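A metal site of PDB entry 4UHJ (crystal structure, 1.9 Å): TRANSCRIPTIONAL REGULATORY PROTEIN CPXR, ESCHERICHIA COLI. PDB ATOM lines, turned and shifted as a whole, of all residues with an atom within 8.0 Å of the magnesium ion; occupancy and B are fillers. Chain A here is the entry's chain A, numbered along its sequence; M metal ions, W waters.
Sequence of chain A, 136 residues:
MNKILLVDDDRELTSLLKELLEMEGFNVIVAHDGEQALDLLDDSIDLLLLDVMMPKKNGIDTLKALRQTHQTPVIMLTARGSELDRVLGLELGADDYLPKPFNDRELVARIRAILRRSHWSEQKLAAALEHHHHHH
The backbone NH (N) of Asp 51 sits at hydrogen-bond distance from the backbone carbonyl oxygen (O) of Val 7 (3.0 Å).
Water W2 bridges OD1 of Asp 8 and NZ of Lys 100.
Of the 16 residues printed, 3 come within 4 Å of the magnesium ion.
Along chain A the residues within 4 Å of the magnesium ion span positions 9 to 53.
The nearest printed residue that does not touch the magnesium ion is Asp 8 (4.005 Å).
OD2 of Asp 51 is bound to the magnesium ion, at 2.2 Å.
O of Met 53 binds the magnesium ion (2.2 Å).
The magnesium ion is bound by OD1 of Asp 9.
Water W1 is bound to the magnesium ion, 2.3 Å away.
Water W2 binds the magnesium ion (2.4 Å).
The magnesium ion has five donor atoms within binding distance.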
ATOM      1  N   VAL A   7      10.309  36.010   4.863  1.00  0.00           N
ATOM      2  CA  VAL A   7       9.831  36.032   6.268  1.00  0.00           C
ATOM      3  C   VAL A   7      10.106  34.694   6.926  1.00  0.00           C
ATOM      4  O   VAL A   7       9.429  33.692   6.624  1.00  0.00           O
ATOM      5  CB  VAL A   7       8.349  36.411   6.402  1.00  0.00           C
ATOM      6  CG1 VAL A   7       7.989  36.653   7.875  1.00  0.00           C
ATOM      7  CG2 VAL A   7       7.970  37.595   5.524  1.00  0.00           C
ATOM      8  N   ASP A   8      11.098  34.675   7.802  1.00  0.00           N
ATOM      9  CA  ASP A   8      11.523  33.462   8.526  1.00  0.00           C
ATOM     10  C   ASP A   8      12.384  33.883   9.698  1.00  0.00           C
ATOM     11  O   ASP A   8      13.181  34.820   9.567  1.00  0.00           O
ATOM     12  CB  ASP A   8      12.307  32.527   7.554  1.00  0.00           C
ATOM     13  CG  ASP A   8      12.446  31.103   8.014  1.00  0.00           C
ATOM     14  OD1 ASP A   8      12.890  30.883   9.161  1.00  0.00           O
ATOM     15  OD2 ASP A   8      12.184  30.184   7.201  1.00  0.00           O
ATOM     16  N   ASP A   9      12.233  33.214  10.844  1.00  0.00           N
ATOM     17  CA  ASP A   9      13.015  33.520  12.056  1.00  0.00           C
ATOM     18  C   ASP A   9      14.428  32.912  11.987  1.00  0.00           C
ATOM     19  O   ASP A   9      15.286  33.342  12.752  1.00  0.00           O
ATOM     20  CB  ASP A   9      12.267  33.038  13.325  1.00  0.00           C
ATOM     21  CG  ASP A   9      11.973  31.548  13.338  1.00  0.00           C
ATOM     22  OD1 ASP A   9      11.348  31.047  12.372  1.00  0.00           O
ATOM     23  OD2 ASP A   9      12.358  30.890  14.307  1.00  0.00           O
ATOM     24  N   ASP A  10      14.669  31.934  11.084  1.00  0.00           N
ATOM     25  CA  ASP A  10      15.996  31.323  10.891  1.00  0.00           C
ATOM     26  C   ASP A  10      16.870  32.311  10.081  1.00  0.00           C
ATOM     27  O   ASP A  10      16.761  32.382   8.846  1.00  0.00           O
ATOM     28  CB  ASP A  10      15.880  29.951  10.195  1.00  0.00           C
ATOM     29  CG  ASP A  10      17.202  29.186   9.985  1.00  0.00           C
ATOM     30  OD1 ASP A  10      18.281  29.757  10.246  1.00  0.00           O
ATOM     31  OD2 ASP A  10      17.142  28.022   9.545  1.00  0.00           O
ATOM     32  N   LEU A  13      19.070  30.722   7.349  1.00  0.00           N
ATOM     33  CA  LEU A  13      18.346  30.480   6.112  1.00  0.00           C
ATOM     34  C   LEU A  13      18.084  31.792   5.336  1.00  0.00           C
ATOM     35  O   LEU A  13      18.289  31.807   4.127  1.00  0.00           O
ATOM     36  CB  LEU A  13      17.015  29.738   6.372  1.00  0.00           C
ATOM     37  CG  LEU A  13      16.119  29.484   5.130  1.00  0.00           C
ATOM     38  CD1 LEU A  13      16.841  28.660   4.048  1.00  0.00           C
ATOM     39  CD2 LEU A  13      14.870  28.826   5.536  1.00  0.00           C
ATOM     40  N   HIS A  32      11.963  38.863  10.319  1.00  0.00           N
ATOM     41  CA  HIS A  32      12.267  37.674  11.109  1.00  0.00           C
ATOM     42  C   HIS A  32      11.065  37.171  11.921  1.00  0.00           C
ATOM     43  O   HIS A  32      11.221  36.225  12.688  1.00  0.00           O
ATOM     44  CB  HIS A  32      13.475  37.897  12.029  1.00  0.00           C
ATOM     45  CG  HIS A  32      14.718  38.334  11.316  1.00  0.00           C
ATOM     46  ND1 HIS A  32      15.140  39.645  11.429  1.00  0.00           N
ATOM     47  CD2 HIS A  32      15.543  37.688  10.457  1.00  0.00           C
ATOM     48  CE1 HIS A  32      16.221  39.746  10.675  1.00  0.00           C
ATOM     49  NE2 HIS A  32      16.516  38.605  10.084  1.00  0.00           N
ATOM     50  N   ASP A  51       7.365  31.621   6.155  1.00  0.00           N
ATOM     51  CA  ASP A  51       7.466  30.511   7.085  1.00  0.00           C
ATOM     52  C   ASP A  51       6.176  30.406   7.911  1.00  0.00           C
ATOM     53  O   ASP A  51       5.372  31.341   7.889  1.00  0.00           O
ATOM     54  CB  ASP A  51       8.702  30.722   8.004  1.00  0.00           C
ATOM     55  CG  ASP A  51       9.064  29.526   8.873  1.00  0.00           C
ATOM     56  OD1 ASP A  51       8.665  28.404   8.528  1.00  0.00           O
ATOM     57  OD2 ASP A  51       9.695  29.731   9.922  1.00  0.00           O
ATOM     58  N   VAL A  52       6.014  29.316   8.663  1.00  0.00           N
ATOM     59  CA  VAL A  52       4.845  29.142   9.528  1.00  0.00           C
ATOM     60  C   VAL A  52       5.249  29.359  10.977  1.00  0.00           C
ATOM     61  O   VAL A  52       4.852  30.389  11.537  1.00  0.00           O
ATOM     62  CB  VAL A  52       4.111  27.792   9.285  1.00  0.00           C
ATOM     63  CG1 VAL A  52       2.974  27.574  10.304  1.00  0.00           C
ATOM     64  CG2 VAL A  52       3.561  27.743   7.853  1.00  0.00           C
ATOM     65  N   MET A  53       6.037  28.434  11.591  1.00  0.00           N
ATOM     66  CA  MET A  53       6.436  28.543  12.994  1.00  0.00           C
ATOM     67  C   MET A  53       7.444  29.664  13.169  1.00  0.00           C
ATOM     68  O   MET A  53       8.608  29.564  12.769  1.00  0.00           O
ATOM     69  CB  MET A  53       7.011  27.202  13.502  1.00  0.00           C
ATOM     70  CG  MET A  53       7.284  27.180  15.008  1.00  0.00           C
ATOM     71  SD  MET A  53       7.956  25.608  15.591  1.00  0.00           S
ATOM     72  CE  MET A  53       6.605  24.513  15.103  1.00  0.00           C
ATOM     73  N   MET A  54       6.983  30.760  13.779  1.00  0.00           N
ATOM     74  CA  MET A  54       7.800  31.936  14.104  1.00  0.00           C
ATOM     75  C   MET A  54       7.343  32.549  15.414  1.00  0.00           C
ATOM     76  O   MET A  54       6.135  32.486  15.717  1.00  0.00           O
ATOM     77  CB  MET A  54       7.676  33.025  13.026  1.00  0.00           C
ATOM     78  CG  MET A  54       8.150  32.632  11.655  1.00  0.00           C
ATOM     79  SD  MET A  54       7.990  34.012  10.491  1.00  0.00           S
ATOM     80  CE  MET A  54       6.200  34.129  10.278  1.00  0.00           C
ATOM     81  N   PRO A  55       8.223  33.237  16.170  1.00  0.00           N
ATOM     82  CA  PRO A  55       7.736  33.915  17.394  1.00  0.00           C
ATOM     83  C   PRO A  55       6.930  35.183  17.036  1.00  0.00           C
ATOM     84  O   PRO A  55       6.947  35.597  15.866  1.00  0.00           O
ATOM     85  CB  PRO A  55       9.030  34.263  18.162  1.00  0.00           C
ATOM     86  CG  PRO A  55      10.107  34.254  17.156  1.00  0.00           C
ATOM     87  CD  PRO A  55       9.681  33.426  15.962  1.00  0.00           C
ATOM     88  N   LEU A  77       7.012  28.649   2.782  1.00  0.00           N
ATOM     89  CA  LEU A  77       8.311  27.932   2.723  1.00  0.00           C
ATOM     90  C   LEU A  77       8.620  27.576   4.149  1.00  0.00           C
ATOM     91  O   LEU A  77       8.966  28.457   4.927  1.00  0.00           O
ATOM     92  CB  LEU A  77       9.390  28.836   2.092  1.00  0.00           C
ATOM     93  CG  LEU A  77      10.777  28.167   1.945  1.00  0.00           C
ATOM     94  CD1 LEU A  77      10.748  27.059   0.857  1.00  0.00           C
ATOM     95  CD2 LEU A  77      11.832  29.192   1.567  1.00  0.00           C
ATOM     96  N   THR A  78       8.364  26.309   4.518  1.00  0.00           N
ATOM     97  CA  THR A  78       8.314  25.919   5.923  1.00  0.00           C
ATOM     98  C   THR A  78       8.593  24.432   6.139  1.00  0.00           C
ATOM     99  O   THR A  78       8.247  23.596   5.279  1.00  0.00           O
ATOM    100  CB  THR A  78       6.844  26.245   6.418  1.00  0.00           C
ATOM    101  OG1 THR A  78       6.572  25.644   7.701  1.00  0.00           O
ATOM    102  CG2 THR A  78       5.762  25.753   5.440  1.00  0.00           C
ATOM    103  N   ALA A  79       9.064  24.083   7.342  1.00  0.00           N
ATOM    104  CA  ALA A  79       9.278  22.688   7.738  1.00  0.00           C
ATOM    105  C   ALA A  79       7.929  21.959   7.968  1.00  0.00           C
ATOM    106  O   ALA A  79       7.911  20.730   8.083  1.00  0.00           O
ATOM    107  CB  ALA A  79      10.136  22.621   9.001  1.00  0.00           C
ATOM    108  N   ARG A  80       6.803  22.708   8.025  1.00  0.00           N
ATOM    109  CA  ARG A  80       5.472  22.107   8.176  1.00  0.00           C
ATOM    110  C   ARG A  80       5.053  21.640   6.799  1.00  0.00           C
ATOM    111  O   ARG A  80       4.409  22.378   6.078  1.00  0.00           O
ATOM    112  CB  ARG A  80       4.488  23.116   8.767  1.00  0.00           C
ATOM    113  CG  ARG A  80       4.790  23.479  10.194  1.00  0.00           C
ATOM    114  CD  ARG A  80       3.509  23.920  10.843  1.00  0.00           C
ATOM    115  NE  ARG A  80       3.401  23.440  12.218  1.00  0.00           N
ATOM    116  CZ  ARG A  80       3.563  24.196  13.293  1.00  0.00           C
ATOM    117  NH1 ARG A  80       3.851  25.488  13.171  1.00  0.00           N
ATOM    118  NH2 ARG A  80       3.436  23.663  14.500  1.00  0.00           N
ATOM    119  N   LYS A 100      10.246  22.524   3.528  1.00  0.00           N
ATOM    120  CA  LYS A 100      11.673  22.404   3.838  1.00  0.00           C
ATOM    121  C   LYS A 100      11.939  20.945   4.226  1.00  0.00           C
ATOM    122  O   LYS A 100      11.083  20.389   4.915  1.00  0.00           O
ATOM    123  CB  LYS A 100      12.105  23.337   4.971  1.00  0.00           C
ATOM    124  CG  LYS A 100      11.957  24.827   4.734  1.00  0.00           C
ATOM    125  CD  LYS A 100      12.447  25.495   6.035  1.00  0.00           C
ATOM    126  CE  LYS A 100      12.161  26.972   6.083  1.00  0.00           C
ATOM    127  NZ  LYS A 100      12.501  27.511   7.438  1.00  0.00           N
HETATM  128 MG    MG M   1      10.549  29.013  11.818  1.00  0.00          MG
HETATM  129  O   HOH W   1      11.329  28.404  13.940  1.00  0.00           O
HETATM  130  O   HOH W   2      12.430  28.545  10.442  1.00  0.00           O
